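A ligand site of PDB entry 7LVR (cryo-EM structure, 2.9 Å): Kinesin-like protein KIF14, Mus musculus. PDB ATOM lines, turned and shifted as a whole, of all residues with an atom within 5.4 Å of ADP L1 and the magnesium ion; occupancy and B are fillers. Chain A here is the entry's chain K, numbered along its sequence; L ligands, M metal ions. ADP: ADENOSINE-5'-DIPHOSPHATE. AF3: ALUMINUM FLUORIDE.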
ATOM      1  N   ARG A  14      -0.495  -2.240  11.259  1.00  0.00           N
ATOM      2  CA  ARG A  14      -1.633  -3.066  10.889  1.00  0.00           C
ATOM      3  C   ARG A  14      -1.310  -4.548  11.043  1.00  0.00           C
ATOM      4  O   ARG A  14      -0.159  -4.972  10.895  1.00  0.00           O
ATOM      5  CB  ARG A  14      -2.072  -2.844   9.443  1.00  0.00           C
ATOM      6  CG  ARG A  14      -2.447  -1.417   9.060  1.00  0.00           C
ATOM      7  CD  ARG A  14      -3.237  -1.395   7.748  1.00  0.00           C
ATOM      8  NE  ARG A  14      -4.554  -2.013   7.870  1.00  0.00           N
ATOM      9  CZ  ARG A  14      -5.434  -2.146   6.883  1.00  0.00           C
ATOM     10  NH1 ARG A  14      -5.169  -1.698   5.661  1.00  0.00           N
ATOM     11  NH2 ARG A  14      -6.604  -2.722   7.100  1.00  0.00           N
ATOM     12  N   VAL A  15      -2.360  -5.321  11.295  1.00  0.00           N
ATOM     13  CA  VAL A  15      -2.312  -6.772  11.295  1.00  0.00           C
ATOM     14  C   VAL A  15      -3.328  -7.281  10.284  1.00  0.00           C
ATOM     15  O   VAL A  15      -4.511  -6.931  10.366  1.00  0.00           O
ATOM     16  CB  VAL A  15      -2.596  -7.373  12.685  1.00  0.00           C
ATOM     17  CG1 VAL A  15      -2.395  -8.869  12.667  1.00  0.00           C
ATOM     18  CG2 VAL A  15      -1.720  -6.723  13.714  1.00  0.00           C
ATOM     19  N   ARG A  16      -2.880  -8.105   9.357  1.00  0.00           N
ATOM     20  CA  ARG A  16      -3.744  -8.623   8.309  1.00  0.00           C
ATOM     21  C   ARG A  16      -4.441  -9.883   8.791  1.00  0.00           C
ATOM     22  O   ARG A  16      -4.131 -10.416   9.855  1.00  0.00           O
ATOM     23  CB  ARG A  16      -2.941  -8.867   7.031  1.00  0.00           C
ATOM     24  CG  ARG A  16      -1.846  -9.933   7.111  1.00  0.00           C
ATOM     25  CD  ARG A  16      -1.498 -10.490   5.744  1.00  0.00           C
ATOM     26  NE  ARG A  16      -0.910 -11.817   5.851  1.00  0.00           N
ATOM     27  CZ  ARG A  16      -0.573 -12.579   4.815  1.00  0.00           C
ATOM     28  NH1 ARG A  16      -0.762 -12.160   3.564  1.00  0.00           N
ATOM     29  NH2 ARG A  16      -0.032 -13.772   5.016  1.00  0.00           N
ATOM     30  N   PRO A  17      -5.410 -10.394   8.032  1.00  0.00           N
ATOM     31  CA  PRO A  17      -6.056 -11.653   8.404  1.00  0.00           C
ATOM     32  C   PRO A  17      -5.187 -12.854   8.058  1.00  0.00           C
ATOM     33  O   PRO A  17      -4.118 -12.752   7.463  1.00  0.00           O
ATOM     34  CB  PRO A  17      -7.345 -11.663   7.578  1.00  0.00           C
ATOM     35  CG  PRO A  17      -7.515 -10.292   7.087  1.00  0.00           C
ATOM     36  CD  PRO A  17      -6.170  -9.717   6.964  1.00  0.00           C
ATOM     37  N   SER A  59      -7.147  -5.611  11.850  1.00  0.00           N
ATOM     38  CA  SER A  59      -8.072  -6.036  10.813  1.00  0.00           C
ATOM     39  C   SER A  59      -8.162  -7.542  10.684  1.00  0.00           C
ATOM     40  O   SER A  59      -8.440  -8.039   9.586  1.00  0.00           O
ATOM     41  CB  SER A  59      -7.648  -5.463   9.463  1.00  0.00           C
ATOM     42  OG  SER A  59      -6.603  -6.243   8.910  1.00  0.00           O
ATOM     43  N   TYR A  67     -12.688  -2.853  15.019  1.00  0.00           N
ATOM     44  CA  TYR A  67     -12.214  -3.291  13.725  1.00  0.00           C
ATOM     45  C   TYR A  67     -11.668  -2.108  12.948  1.00  0.00           C
ATOM     46  O   TYR A  67     -12.399  -1.159  12.649  1.00  0.00           O
ATOM     47  CB  TYR A  67     -13.344  -3.955  12.940  1.00  0.00           C
ATOM     48  CG  TYR A  67     -12.929  -4.578  11.642  1.00  0.00           C
ATOM     49  CD1 TYR A  67     -12.074  -5.670  11.622  1.00  0.00           C
ATOM     50  CD2 TYR A  67     -13.403  -4.103  10.438  1.00  0.00           C
ATOM     51  CE1 TYR A  67     -11.696  -6.253  10.428  1.00  0.00           C
ATOM     52  CE2 TYR A  67     -13.032  -4.674   9.241  1.00  0.00           C
ATOM     53  CZ  TYR A  67     -12.179  -5.753   9.239  1.00  0.00           C
ATOM     54  OH  TYR A  67     -11.797  -6.331   8.053  1.00  0.00           O
ATOM     55  N   GLN A  98       6.375  -7.477   5.293  1.00  0.00           N
ATOM     56  CA  GLN A  98       6.759  -8.708   4.649  1.00  0.00           C
ATOM     57  C   GLN A  98       6.034  -8.850   3.314  1.00  0.00           C
ATOM     58  O   GLN A  98       5.118  -8.092   2.996  1.00  0.00           O
ATOM     59  CB  GLN A  98       6.421  -9.891   5.568  1.00  0.00           C
ATOM     60  CG  GLN A  98       6.978 -11.258   5.182  1.00  0.00           C
ATOM     61  CD  GLN A  98       6.705 -12.293   6.235  1.00  0.00           C
ATOM     62  OE1 GLN A  98       6.006 -12.020   7.205  1.00  0.00           O
ATOM     63  NE2 GLN A  98       7.232 -13.485   6.047  1.00  0.00           N
ATOM     64  N   THR A  99       6.459  -9.828   2.533  1.00  0.00           N
ATOM     65  CA  THR A  99       5.761 -10.178   1.316  1.00  0.00           C
ATOM     66  C   THR A  99       4.368 -10.702   1.665  1.00  0.00           C
ATOM     67  O   THR A  99       4.229 -11.660   2.418  1.00  0.00           O
ATOM     68  CB  THR A  99       6.557 -11.220   0.542  1.00  0.00           C
ATOM     69  OG1 THR A  99       7.946 -10.907   0.609  1.00  0.00           O
ATOM     70  CG2 THR A  99       6.135 -11.250  -0.892  1.00  0.00           C
ATOM     71  N   GLY A 100       3.349 -10.048   1.119  1.00  0.00           N
ATOM     72  CA  GLY A 100       1.977 -10.408   1.391  1.00  0.00           C
ATOM     73  C   GLY A 100       1.436  -9.889   2.693  1.00  0.00           C
ATOM     74  O   GLY A 100       0.348 -10.313   3.110  1.00  0.00           O
ATOM     75  N   SER A 101       2.140  -8.972   3.352  1.00  0.00           N
ATOM     76  CA  SER A 101       1.739  -8.543   4.692  1.00  0.00           C
ATOM     77  C   SER A 101       0.578  -7.562   4.702  1.00  0.00           C
ATOM     78  O   SER A 101       0.101  -7.235   5.789  1.00  0.00           O
ATOM     79  CB  SER A 101       2.937  -7.916   5.406  1.00  0.00           C
ATOM     80  OG  SER A 101       3.549  -6.921   4.608  1.00  0.00           O
ATOM     81  N   GLY A 102       0.113  -7.092   3.546  1.00  0.00           N
ATOM     82  CA  GLY A 102      -1.044  -6.211   3.499  1.00  0.00           C
ATOM     83  C   GLY A 102      -0.704  -4.742   3.305  1.00  0.00           C
ATOM     84  O   GLY A 102      -1.272  -3.877   3.979  1.00  0.00           O
ATOM     85  N   LYS A 103       0.205  -4.456   2.382  1.00  0.00           N
ATOM     86  CA  LYS A 103       0.677  -3.097   2.178  1.00  0.00           C
ATOM     87  C   LYS A 103      -0.076  -2.395   1.056  1.00  0.00           C
ATOM     88  O   LYS A 103      -0.645  -1.321   1.254  1.00  0.00           O
ATOM     89  CB  LYS A 103       2.165  -3.109   1.880  1.00  0.00           C
ATOM     90  CG  LYS A 103       2.992  -3.648   3.013  1.00  0.00           C
ATOM     91  CD  LYS A 103       4.466  -3.604   2.703  1.00  0.00           C
ATOM     92  CE  LYS A 103       4.830  -4.655   1.682  1.00  0.00           C
ATOM     93  NZ  LYS A 103       6.303  -4.882   1.661  1.00  0.00           N
ATOM     94  N   SER A 104      -0.076  -3.000  -0.130  1.00  0.00           N
ATOM     95  CA  SER A 104      -0.808  -2.416  -1.257  1.00  0.00           C
ATOM     96  C   SER A 104      -2.313  -2.481  -1.044  1.00  0.00           C
ATOM     97  O   SER A 104      -3.061  -1.810  -1.769  1.00  0.00           O
ATOM     98  CB  SER A 104      -0.413  -3.127  -2.546  1.00  0.00           C
ATOM     99  OG  SER A 104       0.984  -3.066  -2.746  1.00  0.00           O
ATOM    100  N   TYR A 105      -2.786  -3.264  -0.082  1.00  0.00           N
ATOM    101  CA  TYR A 105      -4.195  -3.232   0.292  1.00  0.00           C
ATOM    102  C   TYR A 105      -4.526  -1.960   1.050  1.00  0.00           C
ATOM    103  O   TYR A 105      -5.671  -1.503   1.029  1.00  0.00           O
ATOM    104  CB  TYR A 105      -4.528  -4.449   1.142  1.00  0.00           C
ATOM    105  CG  TYR A 105      -5.863  -4.422   1.844  1.00  0.00           C
ATOM    106  CD1 TYR A 105      -7.030  -4.803   1.198  1.00  0.00           C
ATOM    107  CD2 TYR A 105      -5.960  -4.018   3.174  1.00  0.00           C
ATOM    108  CE1 TYR A 105      -8.248  -4.784   1.852  1.00  0.00           C
ATOM    109  CE2 TYR A 105      -7.165  -3.999   3.834  1.00  0.00           C
ATOM    110  CZ  TYR A 105      -8.306  -4.386   3.168  1.00  0.00           C
ATOM    111  OH  TYR A 105      -9.518  -4.355   3.825  1.00  0.00           O
ATOM    112  N   LEU A 110      -8.043  -2.048  -3.166  1.00  0.00           N
ATOM    113  CA  LEU A 110      -8.767  -2.740  -4.226  1.00  0.00           C
ATOM    114  C   LEU A 110      -9.993  -1.922  -4.613  1.00  0.00           C
ATOM    115  O   LEU A 110     -10.349  -0.938  -3.965  1.00  0.00           O
ATOM    116  CB  LEU A 110      -9.181  -4.141  -3.754  1.00  0.00           C
ATOM    117  CG  LEU A 110      -9.558  -5.214  -4.777  1.00  0.00           C
ATOM    118  CD1 LEU A 110      -8.494  -5.386  -5.843  1.00  0.00           C
ATOM    119  CD2 LEU A 110      -9.785  -6.536  -4.050  1.00  0.00           C
ATOM    120  N   ARG A 206       2.489  -0.871 -13.186  1.00  0.00           N
ATOM    121  CA  ARG A 206       3.423  -1.294 -12.154  1.00  0.00           C
ATOM    122  C   ARG A 206       3.827  -2.742 -12.363  1.00  0.00           C
ATOM    123  O   ARG A 206       3.057  -3.554 -12.867  1.00  0.00           O
ATOM    124  CB  ARG A 206       2.815  -1.122 -10.773  1.00  0.00           C
ATOM    125  CG  ARG A 206       3.802  -1.227  -9.649  1.00  0.00           C
ATOM    126  CD  ARG A 206       3.170  -0.834  -8.346  1.00  0.00           C
ATOM    127  NE  ARG A 206       3.967  -1.231  -7.194  1.00  0.00           N
ATOM    128  CZ  ARG A 206       3.580  -1.098  -5.926  1.00  0.00           C
ATOM    129  NH1 ARG A 206       2.408  -0.565  -5.621  1.00  0.00           N
ATOM    130  NH2 ARG A 206       4.385  -1.496  -4.974  1.00  0.00           N
ATOM    131  N   ASN A 214       2.310 -14.426  -3.024  1.00  0.00           N
ATOM    132  CA  ASN A 214       1.252 -13.612  -3.618  1.00  0.00           C
ATOM    133  C   ASN A 214       1.113 -13.973  -5.090  1.00  0.00           C
ATOM    134  O   ASN A 214       2.107 -14.142  -5.806  1.00  0.00           O
ATOM    135  CB  ASN A 214       1.529 -12.120  -3.466  1.00  0.00           C
ATOM    136  CG  ASN A 214       1.508 -11.670  -2.023  1.00  0.00           C
ATOM    137  OD1 ASN A 214       2.540 -11.636  -1.355  1.00  0.00           O
ATOM    138  ND2 ASN A 214       0.340 -11.324  -1.539  1.00  0.00           N
ATOM    139  N   LYS A 216      -0.441 -11.898  -7.164  1.00  0.00           N
ATOM    140  CA  LYS A 216      -0.126 -10.602  -7.755  1.00  0.00           C
ATOM    141  C   LYS A 216       0.762  -9.862  -6.770  1.00  0.00           C
ATOM    142  O   LYS A 216       0.296  -9.091  -5.927  1.00  0.00           O
ATOM    143  CB  LYS A 216      -1.391  -9.814  -8.070  1.00  0.00           C
ATOM    144  CG  LYS A 216      -2.147 -10.320  -9.284  1.00  0.00           C
ATOM    145  CD  LYS A 216      -3.142  -9.278  -9.789  1.00  0.00           C
ATOM    146  CE  LYS A 216      -4.238  -8.958  -8.768  1.00  0.00           C
ATOM    147  NZ  LYS A 216      -4.944 -10.164  -8.264  1.00  0.00           N
ATOM    148  N   SER A 217       2.066 -10.109  -6.877  1.00  0.00           N
ATOM    149  CA  SER A 217       3.035  -9.501  -5.989  1.00  0.00           C
ATOM    150  C   SER A 217       3.602  -8.243  -6.608  1.00  0.00           C
ATOM    151  O   SER A 217       3.443  -7.979  -7.808  1.00  0.00           O
ATOM    152  CB  SER A 217       4.171 -10.472  -5.698  1.00  0.00           C
ATOM    153  OG  SER A 217       5.065 -10.527  -6.791  1.00  0.00           O
ATOM    154  N   SER A 218       4.264  -7.451  -5.786  1.00  0.00           N
ATOM    155  CA  SER A 218       4.863  -6.202  -6.206  1.00  0.00           C
ATOM    156  C   SER A 218       6.360  -6.361  -6.374  1.00  0.00           C
ATOM    157  O   SER A 218       7.092  -6.531  -5.396  1.00  0.00           O
ATOM    158  CB  SER A 218       4.557  -5.102  -5.202  1.00  0.00           C
ATOM    159  OG  SER A 218       3.218  -5.160  -4.758  1.00  0.00           O
ATOM    160  N   ASP A 253       4.562   2.838  -1.273  1.00  0.00           N
ATOM    161  CA  ASP A 253       4.362   1.416  -1.019  1.00  0.00           C
ATOM    162  C   ASP A 253       5.585   0.665  -1.507  1.00  0.00           C
ATOM    163  O   ASP A 253       5.946   0.728  -2.689  1.00  0.00           O
ATOM    164  CB  ASP A 253       3.103   0.904  -1.710  1.00  0.00           C
ATOM    165  CG  ASP A 253       2.715  -0.483  -1.244  1.00  0.00           C
ATOM    166  OD1 ASP A 253       3.485  -1.432  -1.481  1.00  0.00           O
ATOM    167  OD2 ASP A 253       1.635  -0.623  -0.635  1.00  0.00           O
ATOM    168  N   LEU A 254       6.207  -0.077  -0.599  1.00  0.00           N
ATOM    169  CA  LEU A 254       7.419  -0.823  -0.863  1.00  0.00           C
ATOM    170  C   LEU A 254       7.115  -2.262  -1.219  1.00  0.00           C
ATOM    171  O   LEU A 254       5.967  -2.724  -1.137  1.00  0.00           O
ATOM    172  CB  LEU A 254       8.328  -0.780   0.347  1.00  0.00           C
ATOM    173  CG  LEU A 254       8.588   0.584   0.962  1.00  0.00           C
ATOM    174  CD1 LEU A 254       9.409   0.444   2.180  1.00  0.00           C
ATOM    175  CD2 LEU A 254       9.267   1.485  -0.011  1.00  0.00           C
HETATM  176  PB  ADP L   1       1.659  -7.197  -1.284  1.00  0.00           P
HETATM  177  O1B ADP L   1       2.215  -6.454  -0.091  1.00  0.00           O
HETATM  178  O2B ADP L   1       1.146  -6.305  -2.388  1.00  0.00           O
HETATM  179  O3B ADP L   1       2.522  -8.329  -1.766  1.00  0.00           O
HETATM  180  PA  ADP L   1      -0.928  -7.008  -0.402  1.00  0.00           P
HETATM  181  O1A ADP L   1      -0.473  -5.979   0.600  1.00  0.00           O
HETATM  182  O2A ADP L   1      -1.512  -6.610  -1.723  1.00  0.00           O
HETATM  183  O3A ADP L   1       0.345  -7.910  -0.715  1.00  0.00           O
HETATM  184  O5' ADP L   1      -1.915  -8.064   0.291  1.00  0.00           O
HETATM  185  C5' ADP L   1      -2.220  -9.235  -0.451  1.00  0.00           C
HETATM  186  C4' ADP L   1      -3.642  -9.707  -0.217  1.00  0.00           C
HETATM  187  O4' ADP L   1      -3.984  -9.543   1.149  1.00  0.00           O
HETATM  188  C3' ADP L   1      -4.665  -8.925  -1.031  1.00  0.00           C
HETATM  189  O3' ADP L   1      -5.211  -9.745  -2.061  1.00  0.00           O
HETATM  190  C2' ADP L   1      -5.728  -8.504  -0.032  1.00  0.00           C
HETATM  191  O2' ADP L   1      -7.034  -8.838  -0.507  1.00  0.00           O
HETATM  192  C1' ADP L   1      -5.384  -9.271   1.223  1.00  0.00           C
HETATM  193  N9  ADP L   1      -5.683  -8.526   2.449  1.00  0.00           N
HETATM  194  C8  ADP L   1      -4.831  -7.732   3.100  1.00  0.00           C
HETATM  195  N7  ADP L   1      -5.417  -7.205   4.195  1.00  0.00           N
HETATM  196  C5  ADP L   1      -6.667  -7.689   4.249  1.00  0.00           C
HETATM  197  C6  ADP L   1      -7.836  -7.546   5.144  1.00  0.00           C
HETATM  198  N6  ADP L   1      -7.757  -6.761   6.241  1.00  0.00           N
HETATM  199  N1  ADP L   1      -8.959  -8.229   4.847  1.00  0.00           N
HETATM  200  C2  ADP L   1      -9.036  -9.017   3.763  1.00  0.00           C
HETATM  201  N3  ADP L   1      -8.021  -9.188   2.903  1.00  0.00           N
HETATM  202  C4  ADP L   1      -6.837  -8.564   3.095  1.00  0.00           C
HETATM  203 AL   AF3 L   2       4.545  -6.876  -1.702  1.00  0.00          AL
HETATM  204  F1  AF3 L   2       4.537  -7.205  -0.033  1.00  0.00           F
HETATM  205  F2  AF3 L   2       3.932  -5.370  -2.246  1.00  0.00           F
HETATM  206  F3  AF3 L   2       4.711  -8.169  -2.805  1.00  0.00           F
HETATM  207 MG    MG M   1       2.157  -4.706  -3.102  1.00  0.00          MG
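N of Gly 100 sits at hydrogen-bond distance from OD1 of Asn 214, 3.0 Å away. N of Ser 104 lies within hydrogen-bond range of OD2 of Asp 253 (3.0 Å). The guanidinium group of Arg 16 sits close to the backbone carbonyl oxygen of Gly 100 (3.4 Å). The guanidinium group (NH2) of Arg 206 lies within salt-bridge range of the side-chain carboxylate (OD1) of Asp 253 (3.6 Å). OG of Ser 59 sits at hydrogen-bond distance from O of Val 15.
The magnesium ion is bound by the side-chain hydroxyl of Ser 218 (2.0 Å), an oxygen (O2B) of ADP L1 (2.0 Å), the side-chain hydroxyl of Ser 104 (2.0 Å) and a fluorine (F2) of AF3 L2 (2.1 Å).
N of Gly 100 sits close to O3B of ADP L1 (3.5 Å). The backbone NH (N) of Ser 218 sits at hydrogen-bond distance from a fluorine (F3) of AF3 L2. N of Gly 100 lies within hydrogen-bond range of F1 of AF3 L2 (3.3 Å). NZ of Lys 103 lies close to F1 of AF3 L2 (3.4 Å). N of Ser 104 is in hydrogen-bond range of O1A of ADP L1. O3B of ADP L1 sits close to OD1 of Asn 214 (3.3 Å). The side-chain hydroxyl (OG) of Ser 59 is in hydrogen-bond range of a nitrogen (N6) of ADP L1. An oxygen (O1A) of ADP L1 lies close to the backbone NH of Gly 102, 3.2 Å away. N of Lys 103 is in hydrogen-bond range of O1A of ADP L1 (2.4 Å).
Merely in contact with ADP L1: Pro 17 (3.3 Å) and Tyr 105 (3.4 Å). Of the 22 residues printed, 9 come within 4 Å of ADP L1. The nearest printed residue that does not touch ADP L1 is Arg 16 (4.1 Å).
Residues that only touch the magnesium ion: Asp 253.
O3B of ADP L1 binds AL of AF3 L2 (2.5 Å).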
